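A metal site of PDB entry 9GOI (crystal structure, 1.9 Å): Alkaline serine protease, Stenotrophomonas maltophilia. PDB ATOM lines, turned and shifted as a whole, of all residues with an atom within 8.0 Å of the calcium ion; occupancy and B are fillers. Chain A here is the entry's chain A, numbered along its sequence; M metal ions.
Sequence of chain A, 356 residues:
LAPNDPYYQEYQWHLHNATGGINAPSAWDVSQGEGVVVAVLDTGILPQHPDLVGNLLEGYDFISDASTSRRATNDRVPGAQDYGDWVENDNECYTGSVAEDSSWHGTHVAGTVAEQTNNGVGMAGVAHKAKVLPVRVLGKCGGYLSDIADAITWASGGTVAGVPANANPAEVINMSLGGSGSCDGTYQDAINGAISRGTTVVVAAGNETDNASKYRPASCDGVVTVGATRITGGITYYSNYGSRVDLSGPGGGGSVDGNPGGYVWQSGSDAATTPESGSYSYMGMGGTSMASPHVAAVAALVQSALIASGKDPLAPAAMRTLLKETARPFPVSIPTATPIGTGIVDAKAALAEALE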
ATOM      1  N   PRO A   3       3.571  13.868   1.056  1.00  0.00           N
ATOM      2  CA  PRO A   3       4.713  13.246   0.372  1.00  0.00           C
ATOM      3  C   PRO A   3       5.534  12.410   1.351  1.00  0.00           C
ATOM      4  O   PRO A   3       5.443  12.624   2.559  1.00  0.00           O
ATOM      5  CB  PRO A   3       5.479  14.448  -0.133  1.00  0.00           C
ATOM      6  CG  PRO A   3       5.194  15.496   0.925  1.00  0.00           C
ATOM      7  CD  PRO A   3       3.708  15.333   1.174  1.00  0.00           C
ATOM      8  N   ASN A   4       6.389  11.547   0.818  1.00  0.00           N
ATOM      9  CA  ASN A   4       7.079  10.545   1.635  1.00  0.00           C
ATOM     10  C   ASN A   4       8.510  10.956   1.997  1.00  0.00           C
ATOM     11  O   ASN A   4       9.279  10.141   2.501  1.00  0.00           O
ATOM     12  CB  ASN A   4       7.138   9.192   0.930  1.00  0.00           C
ATOM     13  CG  ASN A   4       8.035   9.246  -0.288  1.00  0.00           C
ATOM     14  OD1 ASN A   4       8.558  10.320  -0.620  1.00  0.00           O
ATOM     15  ND2 ASN A   4       8.183   8.128  -0.978  1.00  0.00           N
ATOM     16  N   ASP A   5       8.867  12.224   1.793  1.00  0.00           N
ATOM     17  CA  ASP A   5      10.212  12.662   2.111  1.00  0.00           C
ATOM     18  C   ASP A   5      10.459  12.459   3.610  1.00  0.00           C
ATOM     19  O   ASP A   5       9.700  12.973   4.416  1.00  0.00           O
ATOM     20  CB  ASP A   5      10.419  14.109   1.718  1.00  0.00           C
ATOM     21  CG  ASP A   5      10.016  14.408   0.277  1.00  0.00           C
ATOM     22  OD1 ASP A   5       8.797  14.546   0.033  1.00  0.00           O
ATOM     23  OD2 ASP A   5      10.915  14.424  -0.570  1.00  0.00           O
ATOM     24  N   PRO A   6      11.533  11.741   4.004  1.00  0.00           N
ATOM     25  CA  PRO A   6      11.730  11.354   5.399  1.00  0.00           C
ATOM     26  C   PRO A   6      11.669  12.475   6.455  1.00  0.00           C
ATOM     27  O   PRO A   6      11.179  12.237   7.551  1.00  0.00           O
ATOM     28  CB  PRO A   6      13.083  10.628   5.427  1.00  0.00           C
ATOM     29  CG  PRO A   6      13.691  10.821   4.036  1.00  0.00           C
ATOM     30  CD  PRO A   6      12.583  11.222   3.091  1.00  0.00           C
ATOM     31  N   TYR A   7      12.156  13.680   6.142  1.00  0.00           N
ATOM     32  CA  TYR A   7      12.239  14.755   7.117  1.00  0.00           C
ATOM     33  C   TYR A   7      11.079  15.744   7.042  1.00  0.00           C
ATOM     34  O   TYR A   7      11.018  16.696   7.851  1.00  0.00           O
ATOM     35  CB  TYR A   7      13.570  15.473   6.921  1.00  0.00           C
ATOM     36  CG  TYR A   7      14.827  14.687   7.204  1.00  0.00           C
ATOM     37  CD1 TYR A   7      14.896  13.810   8.280  1.00  0.00           C
ATOM     38  CD2 TYR A   7      15.964  14.828   6.418  1.00  0.00           C
ATOM     39  CE1 TYR A   7      16.055  13.119   8.577  1.00  0.00           C
ATOM     40  CE2 TYR A   7      17.128  14.128   6.701  1.00  0.00           C
ATOM     41  CZ  TYR A   7      17.169  13.263   7.782  1.00  0.00           C
ATOM     42  OH  TYR A   7      18.279  12.553   8.104  1.00  0.00           O
ATOM     43  N   TYR A   8      10.153  15.534   6.086  1.00  0.00           N
ATOM     44  CA  TYR A   8       9.079  16.471   5.810  1.00  0.00           C
ATOM     45  C   TYR A   8       8.165  16.642   7.029  1.00  0.00           C
ATOM     46  O   TYR A   8       7.897  17.772   7.454  1.00  0.00           O
ATOM     47  CB  TYR A   8       8.315  16.000   4.561  1.00  0.00           C
ATOM     48  CG  TYR A   8       6.922  16.600   4.388  1.00  0.00           C
ATOM     49  CD1 TYR A   8       6.736  17.871   3.882  1.00  0.00           C
ATOM     50  CD2 TYR A   8       5.796  15.860   4.727  1.00  0.00           C
ATOM     51  CE1 TYR A   8       5.463  18.396   3.702  1.00  0.00           C
ATOM     52  CE2 TYR A   8       4.519  16.357   4.536  1.00  0.00           C
ATOM     53  CZ  TYR A   8       4.355  17.644   4.047  1.00  0.00           C
ATOM     54  OH  TYR A   8       3.082  18.068   3.882  1.00  0.00           O
ATOM     55  N   GLN A  12       9.087  20.276   8.443  1.00  0.00           N
ATOM     56  CA  GLN A  12       8.616  21.313   7.512  1.00  0.00           C
ATOM     57  C   GLN A  12       7.238  21.873   7.849  1.00  0.00           C
ATOM     58  O   GLN A  12       6.339  21.943   7.001  1.00  0.00           O
ATOM     59  CB  GLN A  12       8.744  20.863   6.062  1.00  0.00           C
ATOM     60  CG  GLN A  12      10.194  20.534   5.708  1.00  0.00           C
ATOM     61  CD  GLN A  12      10.366  20.234   4.241  1.00  0.00           C
ATOM     62  OE1 GLN A  12       9.977  19.156   3.757  1.00  0.00           O
ATOM     63  NE2 GLN A  12      10.923  21.189   3.521  1.00  0.00           N
ATOM     64  N   HIS A  49      23.167  18.579  -5.768  1.00  0.00           N
ATOM     65  CA  HIS A  49      22.502  18.160  -4.551  1.00  0.00           C
ATOM     66  C   HIS A  49      21.499  17.079  -4.954  1.00  0.00           C
ATOM     67  O   HIS A  49      20.628  17.321  -5.789  1.00  0.00           O
ATOM     68  CB  HIS A  49      21.874  19.329  -3.791  1.00  0.00           C
ATOM     69  CG  HIS A  49      21.459  18.996  -2.400  1.00  0.00           C
ATOM     70  ND1 HIS A  49      20.485  18.052  -2.117  1.00  0.00           N
ATOM     71  CD2 HIS A  49      21.901  19.440  -1.195  1.00  0.00           C
ATOM     72  CE1 HIS A  49      20.334  17.928  -0.794  1.00  0.00           C
ATOM     73  NE2 HIS A  49      21.187  18.790  -0.208  1.00  0.00           N
ATOM     74  N   PRO A  50      21.565  15.902  -4.305  1.00  0.00           N
ATOM     75  CA  PRO A  50      20.723  14.773  -4.684  1.00  0.00           C
ATOM     76  C   PRO A  50      19.225  15.051  -4.532  1.00  0.00           C
ATOM     77  O   PRO A  50      18.412  14.341  -5.102  1.00  0.00           O
ATOM     78  CB  PRO A  50      21.212  13.634  -3.760  1.00  0.00           C
ATOM     79  CG  PRO A  50      21.874  14.342  -2.581  1.00  0.00           C
ATOM     80  CD  PRO A  50      22.443  15.607  -3.160  1.00  0.00           C
ATOM     81  N   ASP A  51      18.870  16.073  -3.742  1.00  0.00           N
ATOM     82  CA  ASP A  51      17.448  16.370  -3.592  1.00  0.00           C
ATOM     83  C   ASP A  51      17.003  17.527  -4.498  1.00  0.00           C
ATOM     84  O   ASP A  51      15.854  17.962  -4.369  1.00  0.00           O
ATOM     85  CB  ASP A  51      17.038  16.653  -2.155  1.00  0.00           C
ATOM     86  CG  ASP A  51      15.640  16.143  -1.815  1.00  0.00           C
ATOM     87  OD1 ASP A  51      15.181  15.220  -2.540  1.00  0.00           O
ATOM     88  OD2 ASP A  51      15.027  16.636  -0.823  1.00  0.00           O
ATOM     89  N   LEU A  52      17.899  18.041  -5.355  1.00  0.00           N
ATOM     90  CA  LEU A  52      17.594  19.088  -6.324  1.00  0.00           C
ATOM     91  C   LEU A  52      17.730  18.609  -7.774  1.00  0.00           C
ATOM     92  O   LEU A  52      16.989  19.074  -8.650  1.00  0.00           O
ATOM     93  CB  LEU A  52      18.495  20.311  -6.113  1.00  0.00           C
ATOM     94  CG  LEU A  52      18.373  21.093  -4.813  1.00  0.00           C
ATOM     95  CD1 LEU A  52      19.266  22.323  -4.857  1.00  0.00           C
ATOM     96  CD2 LEU A  52      16.932  21.477  -4.491  1.00  0.00           C
ATOM     97  N   ALA A 114      11.707  24.470  -5.306  1.00  0.00           N
ATOM     98  CA  ALA A 114      11.494  23.268  -6.116  1.00  0.00           C
ATOM     99  C   ALA A 114      12.262  22.035  -5.645  1.00  0.00           C
ATOM    100  O   ALA A 114      12.591  21.179  -6.457  1.00  0.00           O
ATOM    101  CB  ALA A 114      11.851  23.570  -7.563  1.00  0.00           C
ATOM    102  N   GLU A 115      12.487  21.856  -4.329  1.00  0.00           N
ATOM    103  CA  GLU A 115      13.126  20.636  -3.865  1.00  0.00           C
ATOM    104  C   GLU A 115      12.311  19.436  -4.346  1.00  0.00           C
ATOM    105  O   GLU A 115      11.086  19.439  -4.267  1.00  0.00           O
ATOM    106  CB  GLU A 115      13.319  20.696  -2.350  1.00  0.00           C
ATOM    107  CG  GLU A 115      14.140  19.545  -1.793  1.00  0.00           C
ATOM    108  CD  GLU A 115      14.908  19.852  -0.533  1.00  0.00           C
ATOM    109  OE1 GLU A 115      14.935  21.011  -0.094  1.00  0.00           O
ATOM    110  OE2 GLU A 115      15.480  18.886   0.019  1.00  0.00           O
ATOM    111  N   GLN A 116      13.009  18.415  -4.844  1.00  0.00           N
ATOM    112  CA  GLN A 116      12.347  17.182  -5.262  1.00  0.00           C
ATOM    113  C   GLN A 116      11.543  16.626  -4.088  1.00  0.00           C
ATOM    114  O   GLN A 116      12.082  16.481  -2.983  1.00  0.00           O
ATOM    115  CB  GLN A 116      13.398  16.194  -5.745  1.00  0.00           C
ATOM    116  CG  GLN A 116      14.054  16.587  -7.069  1.00  0.00           C
ATOM    117  CD  GLN A 116      13.273  16.078  -8.257  1.00  0.00           C
ATOM    118  OE1 GLN A 116      12.064  15.877  -8.171  1.00  0.00           O
ATOM    119  NE2 GLN A 116      13.945  15.908  -9.391  1.00  0.00           N
ATOM    120  N   THR A 117      10.292  16.263  -4.387  1.00  0.00           N
ATOM    121  CA  THR A 117       9.310  15.913  -3.370  1.00  0.00           C
ATOM    122  C   THR A 117       8.714  14.541  -3.680  1.00  0.00           C
ATOM    123  O   THR A 117       8.567  14.135  -4.836  1.00  0.00           O
ATOM    124  CB  THR A 117       8.262  17.011  -3.295  1.00  0.00           C
ATOM    125  OG1 THR A 117       8.929  18.222  -2.918  1.00  0.00           O
ATOM    126  CG2 THR A 117       7.191  16.702  -2.263  1.00  0.00           C
ATOM    127  N   ASN A 118       8.376  13.803  -2.617  1.00  0.00           N
ATOM    128  CA  ASN A 118       7.792  12.486  -2.745  1.00  0.00           C
ATOM    129  C   ASN A 118       8.773  11.552  -3.455  1.00  0.00           C
ATOM    130  O   ASN A 118       8.358  10.639  -4.143  1.00  0.00           O
ATOM    131  CB  ASN A 118       6.418  12.518  -3.395  1.00  0.00           C
ATOM    132  CG  ASN A 118       5.518  11.369  -2.967  1.00  0.00           C
ATOM    133  OD1 ASN A 118       5.578  10.883  -1.836  1.00  0.00           O
ATOM    134  ND2 ASN A 118       4.686  10.915  -3.888  1.00  0.00           N
ATOM    135  N   ASN A 119      10.078  11.773  -3.232  1.00  0.00           N
ATOM    136  CA  ASN A 119      11.135  10.983  -3.832  1.00  0.00           C
ATOM    137  C   ASN A 119      11.856  10.165  -2.761  1.00  0.00           C
ATOM    138  O   ASN A 119      12.894   9.565  -3.019  1.00  0.00           O
ATOM    139  CB  ASN A 119      12.103  11.854  -4.657  1.00  0.00           C
ATOM    140  CG  ASN A 119      12.981  12.738  -3.794  1.00  0.00           C
ATOM    141  OD1 ASN A 119      12.601  13.131  -2.679  1.00  0.00           O
ATOM    142  ND2 ASN A 119      14.152  13.085  -4.296  1.00  0.00           N
ATOM    143  N   GLY A 120      11.290  10.105  -1.554  1.00  0.00           N
ATOM    144  CA  GLY A 120      11.873   9.304  -0.488  1.00  0.00           C
ATOM    145  C   GLY A 120      13.276   9.766  -0.097  1.00  0.00           C
ATOM    146  O   GLY A 120      14.028   8.952   0.429  1.00  0.00           O
ATOM    147  N   VAL A 121      13.567  11.065  -0.256  1.00  0.00           N
ATOM    148  CA  VAL A 121      14.863  11.634   0.069  1.00  0.00           C
ATOM    149  C   VAL A 121      14.679  13.000   0.726  1.00  0.00           C
ATOM    150  O   VAL A 121      13.960  13.851   0.214  1.00  0.00           O
ATOM    151  CB  VAL A 121      15.765  11.781  -1.177  1.00  0.00           C
ATOM    152  CG1 VAL A 121      17.066  12.490  -0.819  1.00  0.00           C
ATOM    153  CG2 VAL A 121      16.065  10.443  -1.822  1.00  0.00           C
ATOM    154  N   GLY A 122      15.300  13.201   1.880  1.00  0.00           N
ATOM    155  CA  GLY A 122      15.443  14.519   2.488  1.00  0.00           C
ATOM    156  C   GLY A 122      14.101  15.214   2.738  1.00  0.00           C
ATOM    157  O   GLY A 122      13.278  14.702   3.489  1.00  0.00           O
ATOM    158  N   MET A 123      13.955  16.418   2.131  1.00  0.00           N
ATOM    159  CA  MET A 123      12.874  17.364   2.426  1.00  0.00           C
ATOM    160  C   MET A 123      11.986  17.528   1.197  1.00  0.00           C
ATOM    161  O   MET A 123      12.291  17.034   0.107  1.00  0.00           O
ATOM    162  CB  MET A 123      13.403  18.766   2.780  1.00  0.00           C
ATOM    163  CG  MET A 123      14.408  18.838   3.919  1.00  0.00           C
ATOM    164  SD  MET A 123      13.518  18.838   5.479  1.00  0.00           S
ATOM    165  CE  MET A 123      14.867  18.691   6.674  1.00  0.00           C
ATOM    166  N   ALA A 124      10.874  18.263   1.368  1.00  0.00           N
ATOM    167  CA  ALA A 124       9.981  18.631   0.272  1.00  0.00           C
ATOM    168  C   ALA A 124      10.233  20.075  -0.176  1.00  0.00           C
ATOM    169  O   ALA A 124      10.898  20.849   0.525  1.00  0.00           O
ATOM    170  CB  ALA A 124       8.534  18.477   0.718  1.00  0.00           C
ATOM    171  N   GLY A 125       9.686  20.417  -1.344  1.00  0.00           N
ATOM    172  CA  GLY A 125       9.616  21.787  -1.833  1.00  0.00           C
ATOM    173  C   GLY A 125       8.206  22.113  -2.327  1.00  0.00           C
ATOM    174  O   GLY A 125       7.396  21.219  -2.581  1.00  0.00           O
ATOM    175  N   HIS A 128       7.437  21.746  -6.752  1.00  0.00           N
ATOM    176  CA  HIS A 128       8.415  20.682  -6.880  1.00  0.00           C
ATOM    177  C   HIS A 128       8.335  19.972  -8.239  1.00  0.00           C
ATOM    178  O   HIS A 128       9.099  19.031  -8.448  1.00  0.00           O
ATOM    179  CB  HIS A 128       8.312  19.713  -5.701  1.00  0.00           C
ATOM    180  CG  HIS A 128       6.959  19.110  -5.493  1.00  0.00           C
ATOM    181  ND1 HIS A 128       6.118  19.395  -4.422  1.00  0.00           N
ATOM    182  CD2 HIS A 128       6.348  18.115  -6.193  1.00  0.00           C
ATOM    183  CE1 HIS A 128       5.034  18.645  -4.516  1.00  0.00           C
ATOM    184  NE2 HIS A 128       5.141  17.863  -5.579  1.00  0.00           N
ATOM    185  N   TYR A 282      20.784  18.908   4.897  1.00  0.00           N
ATOM    186  CA  TYR A 282      19.574  19.731   5.037  1.00  0.00           C
ATOM    187  C   TYR A 282      19.807  20.737   6.168  1.00  0.00           C
ATOM    188  O   TYR A 282      20.337  20.373   7.232  1.00  0.00           O
ATOM    189  CB  TYR A 282      18.336  18.826   5.183  1.00  0.00           C
ATOM    190  CG  TYR A 282      18.313  17.813   4.061  1.00  0.00           C
ATOM    191  CD1 TYR A 282      17.789  18.142   2.802  1.00  0.00           C
ATOM    192  CD2 TYR A 282      18.931  16.579   4.187  1.00  0.00           C
ATOM    193  CE1 TYR A 282      17.805  17.235   1.753  1.00  0.00           C
ATOM    194  CE2 TYR A 282      18.962  15.675   3.140  1.00  0.00           C
ATOM    195  CZ  TYR A 282      18.423  16.014   1.906  1.00  0.00           C
ATOM    196  OH  TYR A 282      18.494  15.148   0.863  1.00  0.00           O
HETATM  197 CA    CA M   1      12.960  15.212  -1.281  1.00  0.00          CA
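Six residues have an atom within 4 Å of the calcium ion: Asp 5, Asp 51, Gln 116, Asn 119, Val 121 and Met 123.
The calcium ion is bound by the backbone carbonyl oxygen (O) of Val 121.
The calcium ion is bound by O of Gln 116 (2.3 Å).
The calcium ion is bound by OD2 of Asp 5, at 2.3 Å.
O of Met 123 binds the calcium ion (2.4 Å).
The side-chain amide oxygen (OD1) of Asn 119 binds the calcium ion (2.5 Å).
OD2 of Asp 51 is bound to the calcium ion, at 2.6 Å.
OD1 of Asp 51 binds the calcium ion, at 2.6 Å.
The calcium ion has seven donor atoms within binding distance.
The side-chain carboxylate of Asp 5 is in hydrogen-bond range of the backbone NH of Asn 118 (2.8 Å).
N of Asn 119 sits at hydrogen-bond distance from OD1 of Asn 4.
OD2 of Asp 51 sits close to OE2 of Glu 115.
N of Asp 51 sits at hydrogen-bond distance from ND1 of His 49, at 3.0 Å.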
